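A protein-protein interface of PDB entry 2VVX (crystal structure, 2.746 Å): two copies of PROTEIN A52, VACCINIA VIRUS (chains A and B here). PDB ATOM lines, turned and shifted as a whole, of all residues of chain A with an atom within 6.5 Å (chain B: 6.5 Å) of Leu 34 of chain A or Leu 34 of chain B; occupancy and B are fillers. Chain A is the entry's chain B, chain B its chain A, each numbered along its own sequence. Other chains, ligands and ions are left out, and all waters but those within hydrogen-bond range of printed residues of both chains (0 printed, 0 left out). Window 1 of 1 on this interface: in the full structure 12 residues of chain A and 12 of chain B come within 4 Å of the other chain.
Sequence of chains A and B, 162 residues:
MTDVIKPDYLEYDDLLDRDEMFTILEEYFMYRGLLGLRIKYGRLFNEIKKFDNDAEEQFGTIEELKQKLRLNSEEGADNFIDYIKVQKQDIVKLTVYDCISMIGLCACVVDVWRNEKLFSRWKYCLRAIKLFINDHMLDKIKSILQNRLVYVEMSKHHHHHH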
ATOM      1  N   LEU A  10      28.513 -15.835 -14.717  1.00  0.00           N
ATOM      2  CA  LEU A  10      27.527 -16.910 -14.847  1.00  0.00           C
ATOM      3  C   LEU A  10      28.127 -18.310 -14.661  1.00  0.00           C
ATOM      4  O   LEU A  10      27.557 -19.138 -13.953  1.00  0.00           O
ATOM      5  CB  LEU A  10      26.817 -16.827 -16.204  1.00  0.00           C
ATOM      6  CG  LEU A  10      25.768 -17.910 -16.459  1.00  0.00           C
ATOM      7  CD1 LEU A  10      24.757 -17.959 -15.321  1.00  0.00           C
ATOM      8  CD2 LEU A  10      25.073 -17.691 -17.788  1.00  0.00           C
ATOM      9  N   PHE A  29      22.038 -11.269 -10.014  1.00  0.00           N
ATOM     10  CA  PHE A  29      20.622 -10.930  -9.979  1.00  0.00           C
ATOM     11  C   PHE A  29      20.058 -10.748 -11.374  1.00  0.00           C
ATOM     12  O   PHE A  29      18.869 -10.976 -11.608  1.00  0.00           O
ATOM     13  CB  PHE A  29      20.373  -9.708  -9.095  1.00  0.00           C
ATOM     14  CG  PHE A  29      20.443 -10.025  -7.626  1.00  0.00           C
ATOM     15  CD1 PHE A  29      19.480 -10.833  -7.034  1.00  0.00           C
ATOM     16  CD2 PHE A  29      21.483  -9.553  -6.844  1.00  0.00           C
ATOM     17  CE1 PHE A  29      19.545 -11.153  -5.686  1.00  0.00           C
ATOM     18  CE2 PHE A  29      21.552  -9.867  -5.502  1.00  0.00           C
ATOM     19  CZ  PHE A  29      20.580 -10.670  -4.921  1.00  0.00           C
ATOM     20  N   MET A  30      20.919 -10.354 -12.305  1.00  0.00           N
ATOM     21  CA  MET A  30      20.519 -10.243 -13.696  1.00  0.00           C
ATOM     22  C   MET A  30      20.232 -11.629 -14.253  1.00  0.00           C
ATOM     23  O   MET A  30      19.175 -11.873 -14.836  1.00  0.00           O
ATOM     24  CB  MET A  30      21.621  -9.587 -14.510  1.00  0.00           C
ATOM     25  CG  MET A  30      21.354  -9.583 -16.001  1.00  0.00           C
ATOM     26  SD  MET A  30      22.763  -8.938 -16.910  1.00  0.00           S
ATOM     27  CE  MET A  30      23.919 -10.295 -16.716  1.00  0.00           C
ATOM     28  N   TYR A  31      21.180 -12.540 -14.060  1.00  0.00           N
ATOM     29  CA  TYR A  31      21.061 -13.881 -14.613  1.00  0.00           C
ATOM     30  C   TYR A  31      19.959 -14.703 -13.944  1.00  0.00           C
ATOM     31  O   TYR A  31      19.149 -15.340 -14.623  1.00  0.00           O
ATOM     32  CB  TYR A  31      22.404 -14.605 -14.560  1.00  0.00           C
ATOM     33  CG  TYR A  31      23.335 -14.197 -15.681  1.00  0.00           C
ATOM     34  CD1 TYR A  31      22.936 -14.306 -17.005  1.00  0.00           C
ATOM     35  CD2 TYR A  31      24.614 -13.710 -15.421  1.00  0.00           C
ATOM     36  CE1 TYR A  31      23.771 -13.944 -18.035  1.00  0.00           C
ATOM     37  CE2 TYR A  31      25.461 -13.343 -16.450  1.00  0.00           C
ATOM     38  CZ  TYR A  31      25.028 -13.463 -17.761  1.00  0.00           C
ATOM     39  OH  TYR A  31      25.849 -13.104 -18.813  1.00  0.00           O
ATOM     40  N   ARG A  32      19.923 -14.689 -12.619  1.00  0.00           N
ATOM     41  CA  ARG A  32      18.891 -15.432 -11.909  1.00  0.00           C
ATOM     42  C   ARG A  32      17.531 -14.799 -12.166  1.00  0.00           C
ATOM     43  O   ARG A  32      16.527 -15.498 -12.317  1.00  0.00           O
ATOM     44  CB  ARG A  32      19.189 -15.479 -10.407  1.00  0.00           C
ATOM     45  CG  ARG A  32      18.053 -16.044  -9.578  1.00  0.00           C
ATOM     46  CD  ARG A  32      18.528 -16.529  -8.221  1.00  0.00           C
ATOM     47  NE  ARG A  32      17.438 -17.140  -7.471  1.00  0.00           N
ATOM     48  CZ  ARG A  32      17.597 -17.858  -6.363  1.00  0.00           C
ATOM     49  NH1 ARG A  32      18.814 -18.072  -5.874  1.00  0.00           N
ATOM     50  NH2 ARG A  32      16.537 -18.374  -5.751  1.00  0.00           N
ATOM     51  N   GLY A  33      17.505 -13.471 -12.223  1.00  0.00           N
ATOM     52  CA  GLY A  33      16.260 -12.745 -12.376  1.00  0.00           C
ATOM     53  C   GLY A  33      15.657 -12.854 -13.765  1.00  0.00           C
ATOM     54  O   GLY A  33      14.454 -12.656 -13.925  1.00  0.00           O
ATOM     55  N   LEU A  34      16.488 -13.164 -14.760  1.00  0.00           N
ATOM     56  CA  LEU A  34      16.050 -13.248 -16.154  1.00  0.00           C
ATOM     57  C   LEU A  34      16.016 -14.683 -16.700  1.00  0.00           C
ATOM     58  O   LEU A  34      15.077 -15.068 -17.393  1.00  0.00           O
ATOM     59  CB  LEU A  34      16.936 -12.373 -17.043  1.00  0.00           C
ATOM     60  CG  LEU A  34      16.953 -10.879 -16.709  1.00  0.00           C
ATOM     61  CD1 LEU A  34      17.834 -10.135 -17.689  1.00  0.00           C
ATOM     62  CD2 LEU A  34      15.542 -10.291 -16.698  1.00  0.00           C
ATOM     63  N   LEU A  35      17.044 -15.466 -16.382  1.00  0.00           N
ATOM     64  CA  LEU A  35      17.139 -16.848 -16.849  1.00  0.00           C
ATOM     65  C   LEU A  35      16.637 -17.856 -15.812  1.00  0.00           C
ATOM     66  O   LEU A  35      16.147 -18.934 -16.151  1.00  0.00           O
ATOM     67  CB  LEU A  35      18.583 -17.187 -17.213  1.00  0.00           C
ATOM     68  CG  LEU A  35      19.253 -16.340 -18.287  1.00  0.00           C
ATOM     69  CD1 LEU A  35      20.692 -16.782 -18.460  1.00  0.00           C
ATOM     70  CD2 LEU A  35      18.485 -16.442 -19.593  1.00  0.00           C
ATOM     71  N   GLY A  36      16.768 -17.523 -14.542  1.00  0.00           N
ATOM     72  CA  GLY A  36      16.365 -18.456 -13.518  1.00  0.00           C
ATOM     73  C   GLY A  36      17.462 -19.453 -13.211  1.00  0.00           C
ATOM     74  O   GLY A  36      18.623 -19.251 -13.581  1.00  0.00           O
ATOM     75  N   VAL A 110      13.409 -12.310  -6.435  1.00  0.00           N
ATOM     76  CA  VAL A 110      13.570 -12.161  -7.873  1.00  0.00           C
ATOM     77  C   VAL A 110      12.942 -13.349  -8.617  1.00  0.00           C
ATOM     78  O   VAL A 110      12.468 -13.199  -9.744  1.00  0.00           O
ATOM     79  CB  VAL A 110      15.051 -11.948  -8.278  1.00  0.00           C
ATOM     80  CG1 VAL A 110      15.728 -13.279  -8.664  1.00  0.00           C
ATOM     81  CG2 VAL A 110      15.126 -10.953  -9.422  1.00  0.00           C
ATOM     82  N   ARG A 114      10.359 -13.031 -11.720  1.00  0.00           N
ATOM     83  CA  ARG A 114      10.647 -13.679 -12.996  1.00  0.00           C
ATOM     84  C   ARG A 114       9.451 -14.514 -13.456  1.00  0.00           C
ATOM     85  O   ARG A 114       9.034 -14.424 -14.611  1.00  0.00           O
ATOM     86  CB  ARG A 114      11.900 -14.551 -12.910  1.00  0.00           C
ATOM     87  CG  ARG A 114      12.362 -15.096 -14.263  1.00  0.00           C
ATOM     88  CD  ARG A 114      13.466 -16.134 -14.110  1.00  0.00           C
ATOM     89  NE  ARG A 114      13.020 -17.272 -13.306  1.00  0.00           N
ATOM     90  CZ  ARG A 114      13.389 -17.508 -12.044  1.00  0.00           C
ATOM     91  NH1 ARG A 114      14.236 -16.689 -11.417  1.00  0.00           N
ATOM     92  NH2 ARG A 114      12.913 -18.577 -11.413  1.00  0.00           N
ATOM     93  N   PHE A 119      10.095  -8.616 -15.476  1.00  0.00           N
ATOM     94  CA  PHE A 119      11.517  -8.865 -15.691  1.00  0.00           C
ATOM     95  C   PHE A 119      12.434  -7.704 -15.337  1.00  0.00           C
ATOM     96  O   PHE A 119      13.605  -7.911 -15.030  1.00  0.00           O
ATOM     97  CB  PHE A 119      11.759  -9.272 -17.138  1.00  0.00           C
ATOM     98  CG  PHE A 119      11.184 -10.603 -17.494  1.00  0.00           C
ATOM     99  CD1 PHE A 119      11.600 -11.749 -16.832  1.00  0.00           C
ATOM    100  CD2 PHE A 119      10.245 -10.720 -18.506  1.00  0.00           C
ATOM    101  CE1 PHE A 119      11.084 -12.991 -17.169  1.00  0.00           C
ATOM    102  CE2 PHE A 119       9.721 -11.956 -18.850  1.00  0.00           C
ATOM    103  CZ  PHE A 119      10.141 -13.094 -18.181  1.00  0.00           C
ATOM    104  N   SER A 120      11.911  -6.485 -15.390  1.00  0.00           N
ATOM    105  CA  SER A 120      12.717  -5.309 -15.088  1.00  0.00           C
ATOM    106  C   SER A 120      12.907  -5.082 -13.580  1.00  0.00           C
ATOM    107  O   SER A 120      13.660  -4.194 -13.171  1.00  0.00           O
ATOM    108  CB  SER A 120      12.084  -4.074 -15.718  1.00  0.00           C
ATOM    109  OG  SER A 120      10.760  -3.906 -15.247  1.00  0.00           O
ATOM    110  N   TRP A 122      14.284  -7.013 -11.366  1.00  0.00           N
ATOM    111  CA  TRP A 122      15.540  -7.515 -10.809  1.00  0.00           C
ATOM    112  C   TRP A 122      16.420  -6.334 -10.373  1.00  0.00           C
ATOM    113  O   TRP A 122      17.212  -6.445  -9.441  1.00  0.00           O
ATOM    114  CB  TRP A 122      16.275  -8.410 -11.816  1.00  0.00           C
ATOM    115  CG  TRP A 122      16.812  -7.656 -12.984  1.00  0.00           C
ATOM    116  CD1 TRP A 122      16.136  -7.310 -14.122  1.00  0.00           C
ATOM    117  CD2 TRP A 122      18.138  -7.137 -13.134  1.00  0.00           C
ATOM    118  NE1 TRP A 122      16.960  -6.610 -14.969  1.00  0.00           N
ATOM    119  CE2 TRP A 122      18.193  -6.488 -14.386  1.00  0.00           C
ATOM    120  CE3 TRP A 122      19.285  -7.159 -12.335  1.00  0.00           C
ATOM    121  CZ2 TRP A 122      19.349  -5.868 -14.853  1.00  0.00           C
ATOM    122  CZ3 TRP A 122      20.434  -6.543 -12.803  1.00  0.00           C
ATOM    123  CH2 TRP A 122      20.457  -5.907 -14.048  1.00  0.00           C
ATOM    124  N   LEU B  10      13.350  -1.909 -21.151  1.00  0.00           N
ATOM    125  CA  LEU B  10      12.566  -3.040 -21.645  1.00  0.00           C
ATOM    126  C   LEU B  10      11.175  -2.645 -22.139  1.00  0.00           C
ATOM    127  O   LEU B  10      10.752  -3.064 -23.218  1.00  0.00           O
ATOM    128  CB  LEU B  10      12.443  -4.129 -20.575  1.00  0.00           C
ATOM    129  CG  LEU B  10      11.663  -5.368 -21.034  1.00  0.00           C
ATOM    130  CD1 LEU B  10      12.210  -5.911 -22.372  1.00  0.00           C
ATOM    131  CD2 LEU B  10      11.676  -6.445 -19.972  1.00  0.00           C
ATOM    132  N   PHE B  29      20.548  -5.611 -25.593  1.00  0.00           N
ATOM    133  CA  PHE B  29      21.237  -6.862 -25.894  1.00  0.00           C
ATOM    134  C   PHE B  29      21.164  -7.827 -24.725  1.00  0.00           C
ATOM    135  O   PHE B  29      21.159  -9.047 -24.916  1.00  0.00           O
ATOM    136  CB  PHE B  29      22.671  -6.608 -26.352  1.00  0.00           C
ATOM    137  CG  PHE B  29      22.749  -6.094 -27.765  1.00  0.00           C
ATOM    138  CD1 PHE B  29      22.407  -6.918 -28.833  1.00  0.00           C
ATOM    139  CD2 PHE B  29      23.119  -4.787 -28.026  1.00  0.00           C
ATOM    140  CE1 PHE B  29      22.445  -6.454 -30.126  1.00  0.00           C
ATOM    141  CE2 PHE B  29      23.165  -4.314 -29.322  1.00  0.00           C
ATOM    142  CZ  PHE B  29      22.826  -5.149 -30.374  1.00  0.00           C
ATOM    143  N   MET B  30      21.070  -7.277 -23.518  1.00  0.00           N
ATOM    144  CA  MET B  30      20.883  -8.089 -22.337  1.00  0.00           C
ATOM    145  C   MET B  30      19.521  -8.759 -22.393  1.00  0.00           C
ATOM    146  O   MET B  30      19.400  -9.972 -22.240  1.00  0.00           O
ATOM    147  CB  MET B  30      20.970  -7.226 -21.090  1.00  0.00           C
ATOM    148  CG  MET B  30      20.678  -7.977 -19.802  1.00  0.00           C
ATOM    149  SD  MET B  30      20.708  -6.832 -18.414  1.00  0.00           S
ATOM    150  CE  MET B  30      19.156  -5.964 -18.662  1.00  0.00           C
ATOM    151  N   TYR B  31      18.489  -7.961 -22.617  1.00  0.00           N
ATOM    152  CA  TYR B  31      17.131  -8.479 -22.602  1.00  0.00           C
ATOM    153  C   TYR B  31      16.850  -9.399 -23.787  1.00  0.00           C
ATOM    154  O   TYR B  31      16.301 -10.488 -23.619  1.00  0.00           O
ATOM    155  CB  TYR B  31      16.116  -7.336 -22.533  1.00  0.00           C
ATOM    156  CG  TYR B  31      15.949  -6.783 -21.139  1.00  0.00           C
ATOM    157  CD1 TYR B  31      15.584  -7.615 -20.090  1.00  0.00           C
ATOM    158  CD2 TYR B  31      16.143  -5.435 -20.870  1.00  0.00           C
ATOM    159  CE1 TYR B  31      15.423  -7.130 -18.810  1.00  0.00           C
ATOM    160  CE2 TYR B  31      15.979  -4.934 -19.587  1.00  0.00           C
ATOM    161  CZ  TYR B  31      15.624  -5.791 -18.559  1.00  0.00           C
ATOM    162  OH  TYR B  31      15.460  -5.316 -17.273  1.00  0.00           O
ATOM    163  N   ARG B  32      17.230  -8.974 -24.988  1.00  0.00           N
ATOM    164  CA  ARG B  32      17.011  -9.814 -26.158  1.00  0.00           C
ATOM    165  C   ARG B  32      17.883 -11.061 -26.084  1.00  0.00           C
ATOM    166  O   ARG B  32      17.443 -12.159 -26.431  1.00  0.00           O
ATOM    167  CB  ARG B  32      17.286  -9.044 -27.447  1.00  0.00           C
ATOM    168  CG  ARG B  32      17.241  -9.918 -28.689  1.00  0.00           C
ATOM    169  CD  ARG B  32      17.058  -9.090 -29.946  1.00  0.00           C
ATOM    170  NE  ARG B  32      16.972  -9.941 -31.130  1.00  0.00           N
ATOM    171  CZ  ARG B  32      16.559  -9.533 -32.324  1.00  0.00           C
ATOM    172  NH1 ARG B  32      16.187  -8.274 -32.508  1.00  0.00           N
ATOM    173  NH2 ARG B  32      16.516 -10.391 -33.333  1.00  0.00           N
ATOM    174  N   GLY B  33      19.116 -10.888 -25.617  1.00  0.00           N
ATOM    175  CA  GLY B  33      20.055 -11.990 -25.526  1.00  0.00           C
ATOM    176  C   GLY B  33      19.726 -13.030 -24.465  1.00  0.00           C
ATOM    177  O   GLY B  33      20.180 -14.169 -24.562  1.00  0.00           O
ATOM    178  N   LEU B  34      18.943 -12.645 -23.456  1.00  0.00           N
ATOM    179  CA  LEU B  34      18.591 -13.547 -22.355  1.00  0.00           C
ATOM    180  C   LEU B  34      17.119 -13.990 -22.357  1.00  0.00           C
ATOM    181  O   LEU B  34      16.814 -15.162 -22.117  1.00  0.00           O
ATOM    182  CB  LEU B  34      18.934 -12.907 -21.005  1.00  0.00           C
ATOM    183  CG  LEU B  34      20.404 -12.513 -20.818  1.00  0.00           C
ATOM    184  CD1 LEU B  34      20.616 -11.904 -19.455  1.00  0.00           C
ATOM    185  CD2 LEU B  34      21.308 -13.712 -21.012  1.00  0.00           C
ATOM    186  N   LEU B  35      16.216 -13.053 -22.629  1.00  0.00           N
ATOM    187  CA  LEU B  35      14.785 -13.344 -22.658  1.00  0.00           C
ATOM    188  C   LEU B  35      14.255 -13.620 -24.070  1.00  0.00           C
ATOM    189  O   LEU B  35      13.276 -14.349 -24.252  1.00  0.00           O
ATOM    190  CB  LEU B  35      14.002 -12.181 -22.058  1.00  0.00           C
ATOM    191  CG  LEU B  35      14.318 -11.791 -20.619  1.00  0.00           C
ATOM    192  CD1 LEU B  35      13.457 -10.596 -20.210  1.00  0.00           C
ATOM    193  CD2 LEU B  35      14.092 -12.979 -19.700  1.00  0.00           C
ATOM    194  N   GLY B  36      14.888 -13.027 -25.072  1.00  0.00           N
ATOM    195  CA  GLY B  36      14.404 -13.189 -26.425  1.00  0.00           C
ATOM    196  C   GLY B  36      13.282 -12.225 -26.752  1.00  0.00           C
ATOM    197  O   GLY B  36      13.091 -11.224 -26.063  1.00  0.00           O
ATOM    198  N   VAL B 110      22.800 -12.556 -31.502  1.00  0.00           N
ATOM    199  CA  VAL B 110      22.498 -12.866 -30.115  1.00  0.00           C
ATOM    200  C   VAL B 110      21.357 -13.890 -30.028  1.00  0.00           C
ATOM    201  O   VAL B 110      21.299 -14.690 -29.092  1.00  0.00           O
ATOM    202  CB  VAL B 110      22.210 -11.583 -29.268  1.00  0.00           C
ATOM    203  CG1 VAL B 110      20.715 -11.278 -29.192  1.00  0.00           C
ATOM    204  CG2 VAL B 110      22.782 -11.746 -27.875  1.00  0.00           C
ATOM    205  N   ARG B 114      21.486 -17.274 -27.789  1.00  0.00           N
ATOM    206  CA  ARG B 114      20.456 -17.554 -26.801  1.00  0.00           C
ATOM    207  C   ARG B 114      19.875 -18.949 -27.005  1.00  0.00           C
ATOM    208  O   ARG B 114      19.751 -19.718 -26.051  1.00  0.00           O
ATOM    209  CB  ARG B 114      19.340 -16.508 -26.850  1.00  0.00           C
ATOM    210  CG  ARG B 114      18.349 -16.606 -25.690  1.00  0.00           C
ATOM    211  CD  ARG B 114      17.153 -15.686 -25.881  1.00  0.00           C
ATOM    212  NE  ARG B 114      16.422 -16.015 -27.105  1.00  0.00           N
ATOM    213  CZ  ARG B 114      16.453 -15.299 -28.228  1.00  0.00           C
ATOM    214  NH1 ARG B 114      17.167 -14.178 -28.302  1.00  0.00           N
ATOM    215  NH2 ARG B 114      15.752 -15.705 -29.276  1.00  0.00           N
ATOM    216  N   PHE B 119      24.601 -18.117 -22.986  1.00  0.00           N
ATOM    217  CA  PHE B 119      23.951 -16.904 -22.498  1.00  0.00           C
ATOM    218  C   PHE B 119      24.883 -15.743 -22.186  1.00  0.00           C
ATOM    219  O   PHE B 119      24.472 -14.589 -22.243  1.00  0.00           O
ATOM    220  CB  PHE B 119      23.117 -17.222 -21.267  1.00  0.00           C
ATOM    221  CG  PHE B 119      21.930 -18.088 -21.555  1.00  0.00           C
ATOM    222  CD1 PHE B 119      20.954 -17.670 -22.448  1.00  0.00           C
ATOM    223  CD2 PHE B 119      21.779 -19.313 -20.920  1.00  0.00           C
ATOM    224  CE1 PHE B 119      19.845 -18.458 -22.706  1.00  0.00           C
ATOM    225  CE2 PHE B 119      20.675 -20.106 -21.176  1.00  0.00           C
ATOM    226  CZ  PHE B 119      19.707 -19.682 -22.069  1.00  0.00           C
ATOM    227  N   SER B 120      26.128 -16.047 -21.848  1.00  0.00           N
ATOM    228  CA  SER B 120      27.094 -15.011 -21.514  1.00  0.00           C
ATOM    229  C   SER B 120      27.658 -14.293 -22.748  1.00  0.00           C
ATOM    230  O   SER B 120      28.396 -13.309 -22.618  1.00  0.00           O
ATOM    231  CB  SER B 120      28.233 -15.610 -20.696  1.00  0.00           C
ATOM    232  OG  SER B 120      28.863 -16.655 -21.409  1.00  0.00           O
ATOM    233  N   TRP B 122      26.109 -12.571 -25.038  1.00  0.00           N
ATOM    234  CA  TRP B 122      25.478 -11.294 -25.351  1.00  0.00           C
ATOM    235  C   TRP B 122      26.463 -10.145 -25.099  1.00  0.00           C
ATOM    236  O   TRP B 122      26.398  -9.104 -25.750  1.00  0.00           O
ATOM    237  CB  TRP B 122      24.188 -11.100 -24.546  1.00  0.00           C
ATOM    238  CG  TRP B 122      24.423 -10.871 -23.093  1.00  0.00           C
ATOM    239  CD1 TRP B 122      24.598 -11.825 -22.131  1.00  0.00           C
ATOM    240  CD2 TRP B 122      24.524  -9.606 -22.425  1.00  0.00           C
ATOM    241  NE1 TRP B 122      24.806 -11.232 -20.901  1.00  0.00           N
ATOM    242  CE2 TRP B 122      24.768  -9.871 -21.057  1.00  0.00           C
ATOM    243  CE3 TRP B 122      24.436  -8.276 -22.847  1.00  0.00           C
ATOM    244  CZ2 TRP B 122      24.920  -8.857 -20.116  1.00  0.00           C
ATOM    245  CZ3 TRP B 122      24.592  -7.267 -21.905  1.00  0.00           C
ATOM    246  CH2 TRP B 122      24.830  -7.565 -20.558  1.00  0.00           C
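The backbone carbonyl oxygen (O) of Tyr 31 of chain B sits at hydrogen-bond distance from the backbone NH (N) of Gly 36 of chain B (3.2 Å). The backbone carbonyl oxygen (O) of Tyr 31 of chain A sits at hydrogen-bond distance from the backbone NH (N) of Gly 36 of chain A (3.2 Å).
Of the 14 printed residues of chain A, 7 touch a printed residue of chain B. Hydrophobic or aromatic side chains of chain A that line the printed part of chain B: Met 30, Tyr 31, Leu 34, Leu 35, Phe 119 and Trp 122. Hydrophobic or aromatic side chains of chain B within 4 Å of the printed part of chain A: Met 30, Tyr 31, Leu 34, Leu 35, Phe 119 and Trp 122. Along chain B the printed residues that touch a printed residue of chain A span positions 30 to 122. Among the printed residues, no Asp or Glu carboxylate lies within 4 Å of a Lys or Arg side-chain nitrogen of the other chain.
OH of Tyr 31 of chain B sits at hydrogen-bond distance from NE1 of Trp 122 of chain A, at 3.0 Å. NE1 of Trp 122 of chain B sits at hydrogen-bond distance from OH of Tyr 31 of chain A. SD of Met 30 of chain A sits close to SD of Met 30 of chain B.
Met 30 of chain A touches Trp 122 of chain B, and with the chains exchanged Trp 122 of chain A touches Met 30 of chain B. Tyr 31 of chain A touches Ser 120 of chain B, and with the chains exchanged Ser 120 of chain A touches Tyr 31 of chain B. Leu 34 of chain B touches its own counterpart, Leu 34 of chain A. Leu 34 of chain A touches Leu 35 of chain B, and with the chains exchanged Leu 35 of chain A touches Leu 34 of chain B. Positions printed for both chains: 10, 29, 30, 31, 32, 33, 34, 35, 36, 110, 114, 119, 120 and 122. Of the 16 pairs that touch across the chains among the printed residues, 16 have their exchanged pair printed and touching as well.
Among the printed residues, pairs that only touch across the chains: Met 30 of chain A with Trp 122 of chain B (3.8 Å), Tyr 31 of chain A with Leu 34 of chain B (3.9 Å), Tyr 31 of chain A with Phe 119 of chain B (3.98 Å), Tyr 31 of chain A with Ser 120 of chain B (3.5 Å), Leu 34 of chain A with Tyr 31 of chain B (3.8 Å), Leu 34 of chain A with Leu 34 of chain B (3.7 Å), Leu 34 of chain A with Leu 35 of chain B (3.3 Å), Leu 35 of chain A with Leu 34 of chain B (3.3 Å), Leu 35 of chain A with Phe 119 of chain B (3.6 Å), Phe 119 of chain A with Tyr 31 of chain B (3.9 Å), Phe 119 of chain A with Leu 35 of chain B (3.5 Å), Ser 120 of chain A with Tyr 31 of chain B (3.5 Å) and Trp 122 of chain A with Met 30 of chain B (3.8 Å).
Of the printed residues of chain B, Leu 34 of chain A touches Tyr 31 (3.8 Å), Leu 34 (3.7 Å) and Leu 35 (3.3 Å). Of the printed residues of chain B, Leu 35 of chain A touches Leu 34 (3.3 Å) and Phe 119 (3.6 Å). Printed residues of chain B within 4 Å of Phe 119 of chain A: Tyr 31 and Leu 35. Leu 34 of chain B touches just these residues of chain A: Tyr 31 (3.9 Å), Leu 34 (3.7 Å) and Leu 35 (3.3 Å). Printed residues of chain A within 4 Å of Phe 119 of chain B: Tyr 31 and Leu 35. Of the printed residues of chain A, Trp 122 of chain B touches Met 30 and Tyr 31. The nearest printed residue of chain A that does not touch Met 30 of chain B is Leu 34 of chain A (4.1 Å).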
